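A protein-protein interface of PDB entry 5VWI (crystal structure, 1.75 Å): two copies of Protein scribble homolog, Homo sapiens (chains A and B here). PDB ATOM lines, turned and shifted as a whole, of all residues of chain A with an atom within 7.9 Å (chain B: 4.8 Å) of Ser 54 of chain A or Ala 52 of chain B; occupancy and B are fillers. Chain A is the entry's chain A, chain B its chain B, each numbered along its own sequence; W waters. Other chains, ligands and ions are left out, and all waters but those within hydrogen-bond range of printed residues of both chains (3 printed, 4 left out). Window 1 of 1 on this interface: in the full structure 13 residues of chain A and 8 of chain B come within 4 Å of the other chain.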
ATOM      1  N   GLU A   8       6.255  23.587  29.088  1.00  0.00           N
ATOM      2  CA  GLU A   8       5.884  24.993  29.142  1.00  0.00           C
ATOM      3  C   GLU A   8       4.716  25.171  28.198  1.00  0.00           C
ATOM      4  O   GLU A   8       4.839  24.873  27.008  1.00  0.00           O
ATOM      5  CB  GLU A   8       7.035  25.910  28.757  1.00  0.00           C
ATOM      6  CG  GLU A   8       6.649  27.383  28.707  1.00  0.00           C
ATOM      7  CD  GLU A   8       7.792  28.248  28.189  1.00  0.00           C
ATOM      8  OE1 GLU A   8       8.708  28.584  28.969  1.00  0.00           O
ATOM      9  OE2 GLU A   8       7.778  28.546  26.987  1.00  0.00           O
ATOM     10  N   ILE A   9       3.596  25.632  28.742  1.00  0.00           N
ATOM     11  CA  ILE A   9       2.386  25.938  27.986  1.00  0.00           C
ATOM     12  C   ILE A   9       2.163  27.451  28.079  1.00  0.00           C
ATOM     13  O   ILE A   9       1.975  27.983  29.173  1.00  0.00           O
ATOM     14  CB  ILE A   9       1.171  25.194  28.548  1.00  0.00           C
ATOM     15  CG1 ILE A   9       1.450  23.691  28.772  1.00  0.00           C
ATOM     16  CG2 ILE A   9      -0.089  25.496  27.693  1.00  0.00           C
ATOM     17  CD1 ILE A   9       1.816  22.940  27.512  1.00  0.00           C
ATOM     18  N   ARG A  10       2.139  28.141  26.955  1.00  0.00           N
ATOM     19  CA  ARG A  10       2.040  29.606  26.976  1.00  0.00           C
ATOM     20  C   ARG A  10       0.745  30.068  26.325  1.00  0.00           C
ATOM     21  O   ARG A  10       0.436  29.691  25.187  1.00  0.00           O
ATOM     22  CB  ARG A  10       3.249  30.256  26.290  1.00  0.00           C
ATOM     23  CG  ARG A  10       4.572  29.818  26.904  1.00  0.00           C
ATOM     24  CD  ARG A  10       5.625  30.896  26.708  1.00  0.00           C
ATOM     25  NE  ARG A  10       5.711  31.344  25.324  1.00  0.00           N
ATOM     26  CZ  ARG A  10       6.532  30.846  24.401  1.00  0.00           C
ATOM     27  NH1 ARG A  10       7.382  29.878  24.687  1.00  0.00           N
ATOM     28  NH2 ARG A  10       6.517  31.345  23.170  1.00  0.00           N
ATOM     29  N   LEU A  11       0.020  30.925  27.038  1.00  0.00           N
ATOM     30  CA  LEU A  11      -1.265  31.447  26.578  1.00  0.00           C
ATOM     31  C   LEU A  11      -1.074  32.885  26.124  1.00  0.00           C
ATOM     32  O   LEU A  11      -0.779  33.746  26.971  1.00  0.00           O
ATOM     33  CB  LEU A  11      -2.305  31.413  27.696  1.00  0.00           C
ATOM     34  CG  LEU A  11      -2.991  30.090  28.017  1.00  0.00           C
ATOM     35  CD1 LEU A  11      -1.987  29.014  28.336  1.00  0.00           C
ATOM     36  CD2 LEU A  11      -4.016  30.260  29.173  1.00  0.00           C
ATOM     37  N   PRO A  12      -1.229  33.202  24.851  1.00  0.00           N
ATOM     38  CA  PRO A  12      -1.143  34.607  24.446  1.00  0.00           C
ATOM     39  C   PRO A  12      -2.417  35.308  24.839  1.00  0.00           C
ATOM     40  O   PRO A  12      -3.449  35.180  24.178  1.00  0.00           O
ATOM     41  CB  PRO A  12      -0.993  34.526  22.933  1.00  0.00           C
ATOM     42  CG  PRO A  12      -1.756  33.358  22.579  1.00  0.00           C
ATOM     43  CD  PRO A  12      -1.481  32.341  23.689  1.00  0.00           C
ATOM     44  N   ARG A  13      -2.351  36.071  25.904  1.00  0.00           N
ATOM     45  CA  ARG A  13      -3.564  36.628  26.460  1.00  0.00           C
ATOM     46  C   ARG A  13      -4.100  37.777  25.615  1.00  0.00           C
ATOM     47  O   ARG A  13      -3.387  38.722  25.263  1.00  0.00           O
ATOM     48  CB  ARG A  13      -3.297  37.095  27.882  1.00  0.00           C
ATOM     49  CG  ARG A  13      -3.341  35.976  28.847  1.00  0.00           C
ATOM     50  CD  ARG A  13      -3.075  36.473  30.231  1.00  0.00           C
ATOM     51  NE  ARG A  13      -1.725  37.025  30.422  1.00  0.00           N
ATOM     52  CZ  ARG A  13      -1.320  37.488  31.593  1.00  0.00           C
ATOM     53  NH1 ARG A  13      -2.158  37.462  32.621  1.00  0.00           N
ATOM     54  NH2 ARG A  13      -0.096  37.949  31.757  1.00  0.00           N
ATOM     55  N   LEU A  18      -9.297  33.243  30.490  1.00  0.00           N
ATOM     56  CA  LEU A  18      -8.318  32.204  30.173  1.00  0.00           C
ATOM     57  C   LEU A  18      -8.962  30.903  29.703  1.00  0.00           C
ATOM     58  O   LEU A  18      -8.346  30.132  28.952  1.00  0.00           O
ATOM     59  CB  LEU A  18      -7.465  31.910  31.403  1.00  0.00           C
ATOM     60  CG  LEU A  18      -6.668  33.078  31.947  1.00  0.00           C
ATOM     61  CD1 LEU A  18      -5.777  32.522  33.027  1.00  0.00           C
ATOM     62  CD2 LEU A  18      -5.827  33.804  30.890  1.00  0.00           C
ATOM     63  N   VAL A  45     -10.916  22.766  31.005  1.00  0.00           N
ATOM     64  CA  VAL A  45     -10.467  23.600  29.905  1.00  0.00           C
ATOM     65  C   VAL A  45     -11.655  23.806  28.976  1.00  0.00           C
ATOM     66  O   VAL A  45     -12.181  22.824  28.434  1.00  0.00           O
ATOM     67  CB  VAL A  45      -9.295  22.923  29.165  1.00  0.00           C
ATOM     68  CG1 VAL A  45      -8.970  23.634  27.941  1.00  0.00           C
ATOM     69  CG2 VAL A  45      -8.040  22.836  30.102  1.00  0.00           C
ATOM     70  N   GLY A  49     -11.830  27.820  24.209  1.00  0.00           N
ATOM     71  CA  GLY A  49     -11.209  28.927  24.900  1.00  0.00           C
ATOM     72  C   GLY A  49      -9.705  28.984  24.694  1.00  0.00           C
ATOM     73  O   GLY A  49      -9.101  28.143  24.037  1.00  0.00           O
ATOM     74  N   LEU A  50      -9.090  29.989  25.320  1.00  0.00           N
ATOM     75  CA  LEU A  50      -7.668  30.292  25.100  1.00  0.00           C
ATOM     76  C   LEU A  50      -6.768  29.168  25.591  1.00  0.00           C
ATOM     77  O   LEU A  50      -5.801  28.761  24.921  1.00  0.00           O
ATOM     78  CB  LEU A  50      -7.325  31.581  25.828  1.00  0.00           C
ATOM     79  CG  LEU A  50      -5.869  32.015  25.746  1.00  0.00           C
ATOM     80  CD1 LEU A  50      -5.417  32.193  24.317  1.00  0.00           C
ATOM     81  CD2 LEU A  50      -5.677  33.290  26.506  1.00  0.00           C
ATOM     82  N   ALA A  51      -7.040  28.683  26.786  1.00  0.00           N
ATOM     83  CA  ALA A  51      -6.185  27.629  27.346  1.00  0.00           C
ATOM     84  C   ALA A  51      -6.204  26.386  26.466  1.00  0.00           C
ATOM     85  O   ALA A  51      -5.161  25.785  26.210  1.00  0.00           O
ATOM     86  CB  ALA A  51      -6.638  27.298  28.770  1.00  0.00           C
ATOM     87  N   ALA A  52      -7.391  25.972  26.008  1.00  0.00           N
ATOM     88  CA  ALA A  52      -7.470  24.816  25.121  1.00  0.00           C
ATOM     89  C   ALA A  52      -6.693  25.040  23.839  1.00  0.00           C
ATOM     90  O   ALA A  52      -5.999  24.144  23.368  1.00  0.00           O
ATOM     91  CB  ALA A  52      -8.944  24.486  24.778  1.00  0.00           C
ATOM     92  N   ARG A  53      -6.816  26.219  23.238  1.00  0.00           N
ATOM     93  CA  ARG A  53      -6.173  26.453  21.959  1.00  0.00           C
ATOM     94  C   ARG A  53      -4.660  26.440  22.106  1.00  0.00           C
ATOM     95  O   ARG A  53      -3.952  26.206  21.127  1.00  0.00           O
ATOM     96  CB  ARG A  53      -6.611  27.803  21.365  1.00  0.00           C
ATOM     97  CG  ARG A  53      -8.080  27.849  20.965  1.00  0.00           C
ATOM     98  CD  ARG A  53      -8.389  29.063  20.071  1.00  0.00           C
ATOM     99  NE  ARG A  53      -7.967  30.303  20.717  1.00  0.00           N
ATOM    100  CZ  ARG A  53      -8.726  31.004  21.557  1.00  0.00           C
ATOM    101  NH1 ARG A  53      -9.971  30.625  21.848  1.00  0.00           N
ATOM    102  NH2 ARG A  53      -8.243  32.100  22.103  1.00  0.00           N
ATOM    103  N   SER A  54      -4.180  26.786  23.284  1.00  0.00           N
ATOM    104  CA  SER A  54      -2.755  26.920  23.606  1.00  0.00           C
ATOM    105  C   SER A  54      -2.128  25.611  24.090  1.00  0.00           C
ATOM    106  O   SER A  54      -0.942  25.599  24.469  1.00  0.00           O
ATOM    107  CB  SER A  54      -2.566  27.978  24.700  1.00  0.00           C
ATOM    108  OG  SER A  54      -3.124  29.255  24.345  1.00  0.00           O
ATOM    109  N   GLY A  55      -2.912  24.538  24.167  1.00  0.00           N
ATOM    110  CA  GLY A  55      -2.393  23.231  24.544  1.00  0.00           C
ATOM    111  C   GLY A  55      -2.458  22.867  26.012  1.00  0.00           C
ATOM    112  O   GLY A  55      -1.895  21.842  26.404  1.00  0.00           O
ATOM    113  N   LEU A  56      -3.149  23.639  26.830  1.00  0.00           N
ATOM    114  CA  LEU A  56      -3.318  23.270  28.229  1.00  0.00           C
ATOM    115  C   LEU A  56      -4.311  22.109  28.316  1.00  0.00           C
ATOM    116  O   LEU A  56      -5.255  22.029  27.541  1.00  0.00           O
ATOM    117  CB  LEU A  56      -3.799  24.466  29.037  1.00  0.00           C
ATOM    118  CG  LEU A  56      -3.590  24.437  30.544  1.00  0.00           C
ATOM    119  CD1 LEU A  56      -2.083  24.435  30.955  1.00  0.00           C
ATOM    120  CD2 LEU A  56      -4.303  25.578  31.206  1.00  0.00           C
ATOM    121  N   ARG A  57      -4.096  21.218  29.288  1.00  0.00           N
ATOM    122  CA  ARG A  57      -4.848  19.967  29.366  1.00  0.00           C
ATOM    123  C   ARG A  57      -5.303  19.661  30.787  1.00  0.00           C
ATOM    124  O   ARG A  57      -4.551  19.870  31.735  1.00  0.00           O
ATOM    125  CB  ARG A  57      -3.994  18.841  28.845  1.00  0.00           C
ATOM    126  CG  ARG A  57      -3.636  18.953  27.330  1.00  0.00           C
ATOM    127  CD  ARG A  57      -4.793  18.734  26.370  1.00  0.00           C
ATOM    128  NE  ARG A  57      -4.484  19.261  25.035  1.00  0.00           N
ATOM    129  CZ  ARG A  57      -3.593  18.724  24.193  1.00  0.00           C
ATOM    130  NH1 ARG A  57      -3.351  19.291  23.013  1.00  0.00           N
ATOM    131  NH2 ARG A  57      -2.959  17.614  24.523  1.00  0.00           N
ATOM    132  N   LEU A  89       1.037  34.415  29.257  1.00  0.00           N
ATOM    133  CA  LEU A  89       0.884  33.680  30.498  1.00  0.00           C
ATOM    134  C   LEU A  89       1.544  32.335  30.303  1.00  0.00           C
ATOM    135  O   LEU A  89       1.036  31.483  29.562  1.00  0.00           O
ATOM    136  CB  LEU A  89      -0.574  33.533  30.897  1.00  0.00           C
ATOM    137  CG  LEU A  89      -0.739  32.913  32.287  1.00  0.00           C
ATOM    138  CD1 LEU A  89      -0.263  33.870  33.356  1.00  0.00           C
ATOM    139  CD2 LEU A  89      -2.196  32.543  32.514  1.00  0.00           C
ATOM    140  N   VAL B  45      -4.592  24.978  14.090  1.00  0.00           N
ATOM    141  CA  VAL B  45      -3.929  24.178  15.112  1.00  0.00           C
ATOM    142  C   VAL B  45      -5.023  23.570  15.981  1.00  0.00           C
ATOM    143  O   VAL B  45      -5.784  24.301  16.629  1.00  0.00           O
ATOM    144  CB  VAL B  45      -2.951  25.007  15.971  1.00  0.00           C
ATOM    145  CG1 VAL B  45      -2.384  24.125  17.113  1.00  0.00           C
ATOM    146  CG2 VAL B  45      -1.801  25.508  15.105  1.00  0.00           C
ATOM    147  N   LEU B  46      -5.124  22.253  15.983  1.00  0.00           N
ATOM    148  CA  LEU B  46      -6.205  21.607  16.700  1.00  0.00           C
ATOM    149  C   LEU B  46      -5.918  21.660  18.196  1.00  0.00           C
ATOM    150  O   LEU B  46      -4.844  21.213  18.630  1.00  0.00           O
ATOM    151  CB  LEU B  46      -6.378  20.147  16.256  1.00  0.00           C
ATOM    152  CG  LEU B  46      -6.673  19.983  14.770  1.00  0.00           C
ATOM    153  CD1 LEU B  46      -6.753  18.490  14.394  1.00  0.00           C
ATOM    154  CD2 LEU B  46      -7.949  20.713  14.378  1.00  0.00           C
ATOM    155  N   PRO B  47      -6.860  22.149  19.004  1.00  0.00           N
ATOM    156  CA  PRO B  47      -6.610  22.310  20.443  1.00  0.00           C
ATOM    157  C   PRO B  47      -6.152  21.049  21.141  1.00  0.00           C
ATOM    158  O   PRO B  47      -5.297  21.122  22.028  1.00  0.00           O
ATOM    159  CB  PRO B  47      -7.971  22.773  20.979  1.00  0.00           C
ATOM    160  CG  PRO B  47      -8.604  23.471  19.808  1.00  0.00           C
ATOM    161  CD  PRO B  47      -8.123  22.778  18.580  1.00  0.00           C
ATOM    162  N   GLY B  49      -4.552  18.545  19.821  1.00  0.00           N
ATOM    163  CA  GLY B  49      -3.525  17.880  19.046  1.00  0.00           C
ATOM    164  C   GLY B  49      -2.122  18.154  19.582  1.00  0.00           C
ATOM    165  O   GLY B  49      -1.918  18.941  20.505  1.00  0.00           O
ATOM    166  N   LEU B  50      -1.133  17.501  18.957  1.00  0.00           N
ATOM    167  CA  LEU B  50       0.247  17.599  19.440  1.00  0.00           C
ATOM    168  C   LEU B  50       0.847  18.971  19.186  1.00  0.00           C
ATOM    169  O   LEU B  50       1.657  19.467  19.992  1.00  0.00           O
ATOM    170  CB  LEU B  50       1.125  16.534  18.776  1.00  0.00           C
ATOM    171  CG  LEU B  50       0.883  15.116  19.270  1.00  0.00           C
ATOM    172  CD1 LEU B  50       1.671  14.126  18.403  1.00  0.00           C
ATOM    173  CD2 LEU B  50       1.275  15.001  20.719  1.00  0.00           C
ATOM    174  N   ALA B  51       0.512  19.563  18.044  1.00  0.00           N
ATOM    175  CA  ALA B  51       1.034  20.891  17.719  1.00  0.00           C
ATOM    176  C   ALA B  51       0.622  21.907  18.783  1.00  0.00           C
ATOM    177  O   ALA B  51       1.438  22.711  19.234  1.00  0.00           O
ATOM    178  CB  ALA B  51       0.511  21.315  16.343  1.00  0.00           C
ATOM    179  N   ALA B  52      -0.671  21.894  19.176  1.00  0.00           N
ATOM    180  CA  ALA B  52      -1.128  22.803  20.233  1.00  0.00           C
ATOM    181  C   ALA B  52      -0.335  22.577  21.506  1.00  0.00           C
ATOM    182  O   ALA B  52       0.165  23.530  22.138  1.00  0.00           O
ATOM    183  CB  ALA B  52      -2.626  22.625  20.503  1.00  0.00           C
ATOM    184  N   ARG B  53      -0.215  21.297  21.907  1.00  0.00           N
ATOM    185  CA  ARG B  53       0.522  20.963  23.117  1.00  0.00           C
ATOM    186  C   ARG B  53       1.954  21.421  23.037  1.00  0.00           C
ATOM    187  O   ARG B  53       2.502  21.902  24.032  1.00  0.00           O
ATOM    188  CB  ARG B  53       0.477  19.451  23.389  1.00  0.00           C
ATOM    189  CG  ARG B  53       1.110  19.064  24.684  1.00  0.00           C
ATOM    190  CD  ARG B  53       0.395  19.622  25.854  1.00  0.00           C
ATOM    191  NE  ARG B  53       0.893  19.105  27.130  1.00  0.00           N
ATOM    192  CZ  ARG B  53       0.343  19.374  28.299  1.00  0.00           C
ATOM    193  NH1 ARG B  53      -0.748  20.140  28.357  1.00  0.00           N
ATOM    194  NH2 ARG B  53       0.853  18.856  29.414  1.00  0.00           N
ATOM    195  N   SER B  54       2.558  21.356  21.850  1.00  0.00           N
ATOM    196  CA  SER B  54       3.963  21.720  21.741  1.00  0.00           C
ATOM    197  C   SER B  54       4.207  23.207  21.695  1.00  0.00           C
ATOM    198  O   SER B  54       5.353  23.619  21.815  1.00  0.00           O
ATOM    199  CB  SER B  54       4.556  21.108  20.510  1.00  0.00           C
ATOM    200  OG  SER B  54       4.392  19.691  20.578  1.00  0.00           O
ATOM    201  N   GLY B  55       3.187  24.008  21.506  1.00  0.00           N
ATOM    202  CA  GLY B  55       3.331  25.457  21.477  1.00  0.00           C
ATOM    203  C   GLY B  55       3.103  26.143  20.149  1.00  0.00           C
ATOM    204  O   GLY B  55       3.343  27.355  20.057  1.00  0.00           O
ATOM    205  N   LEU B  56       2.666  25.441  19.117  1.00  0.00           N
ATOM    206  CA  LEU B  56       2.454  26.076  17.827  1.00  0.00           C
ATOM    207  C   LEU B  56       1.132  26.812  17.795  1.00  0.00           C
ATOM    208  O   LEU B  56       0.162  26.426  18.479  1.00  0.00           O
ATOM    209  CB  LEU B  56       2.477  25.017  16.727  1.00  0.00           C
ATOM    210  CG  LEU B  56       3.880  24.438  16.499  1.00  0.00           C
ATOM    211  CD1 LEU B  56       3.786  23.227  15.537  1.00  0.00           C
ATOM    212  CD2 LEU B  56       4.781  25.504  15.904  1.00  0.00           C
HETATM  213  O   HOH W   1      -0.963  16.434  22.492  1.00  0.00           O
HETATM  214  O   HOH W   2      -5.642  25.400  18.960  1.00  0.00           O
HETATM  215  O   HOH W   3      -2.397  27.241  19.221  1.00  0.00           O
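O of Ser 54 of chain A lies close to O of Ala 52 of chain B, at 3.3 Å. O of Gly 55 of chain A lies within hydrogen-bond range of NH1 of Arg 53 of chain B (2.8 Å). The backbone carbonyl oxygen (O) of Pro 47 of chain B is in hydrogen-bond range of the guanidinium group (NH1) of Arg 57 of chain A. O of Ala 52 of chain A sits close to O of Pro 47 of chain B. The guanidinium group (NH1) of Arg 57 of chain A is in hydrogen-bond range of the backbone carbonyl oxygen (O) of Gly 49 of chain B (2.9 Å).
The side-chain hydroxyl (OG) of Ser 54 of chain A is in hydrogen-bond range of the backbone carbonyl oxygen (O) of Leu 50 of chain A, 2.8 Å away. O of Gly 49 of chain A sits close to NH1 of Arg 53 of chain A (3.4 Å).
Among the printed residues, merely in contact across the chains: Arg 57 of chain A with Arg 53 of chain B (3.3 Å), Gly 55 of chain A with Ala 52 of chain B (3.5 Å), Ile 9 of chain A with Arg 53 of chain B (3.7 Å) and Arg 53 of chain A with Ala 52 of chain B (3.9 Å).
Printed residues of chain B within 4 Å of Arg 53 of chain A: Ala 52. Of chain B, only Ala 52 (3.3 Å) comes within 4 Å of Ser 54 of chain A. Of the printed residues of chain B, Gly 55 of chain A touches Ala 52 and Arg 53. Of the printed residues of chain B, Arg 57 of chain A touches Pro 47 (2.8 Å), Gly 49 (2.9 Å) and Arg 53 (3.3 Å). Val 45 of chain B touches none of the printed residues of chain A. Of the printed residues of chain A, Pro 47 of chain B touches Ala 52 (3.4 Å) and Arg 57 (2.8 Å). Printed residues of chain A within 4 Å of Gly 49 of chain B: Arg 57. Leu 50 of chain B touches none of the printed residues of chain A. No residue of chain A comes within 4 Å of Ala 51 of chain B. Of chain A, only Arg 53, Ser 54 and Gly 55 come within 4 Å of Ala 52 of chain B. The nearest printed residue of chain B that does not touch Ile 9 of chain A is Ala 52 of chain B (5.7 Å).
Of the 11 printed residues of chain B, 4 touch a printed residue of chain A. Hydrophobic or aromatic side chains of chain B within 4 Å of the printed part of chain A: Pro 47 and Ala 52. Printed residues of chain A that touch a printed residue of chain B: Ile 9, Ala 52, Arg 53, Ser 54, Gly 55 and Arg 57. Hydrophobic or aromatic side chains of chain A within 4 Å of the printed part of chain B: Ile 9. Among the printed residues, 9 pairs touch across the chains.
Arg 53 of chain A touches Ala 52 of chain B, but with the chains exchanged Ala 52 of chain A does not touch Arg 53 of chain B (6.6 Å). Ser 54 of chain A touches Ala 52 of chain B, but with the chains exchanged Ala 52 of chain A does not touch Ser 54 of chain B (9.1 Å). Gly 55 of chain A touches Ala 52 of chain B, but with the chains exchanged Ala 52 of chain A does not touch Gly 55 of chain B (9.4 Å). Gly 55 of chain A touches Arg 53 of chain B, but with the chains exchanged Arg 53 of chain A does not touch Gly 55 of chain B (7.1 Å). Of the 9 pairs that touch across the chains among the printed residues, none has its exchanged pair printed and touching as well.
Water W2 lies within hydrogen-bond range of O of Val 45 of chain B (2.6 Å) and O of Arg 53 of chain A (2.9 Å). Water W3 bridges the backbone carbonyl oxygen (O) of Arg 53 of chain A (2.7 Å) and the backbone carbonyl oxygen (O) of Leu 56 of chain B (2.8 Å). Water W1 bridges NH2 of Arg 57 of chain A (3.1 Å) and O of Gly 49 of chain B (3.3 Å).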
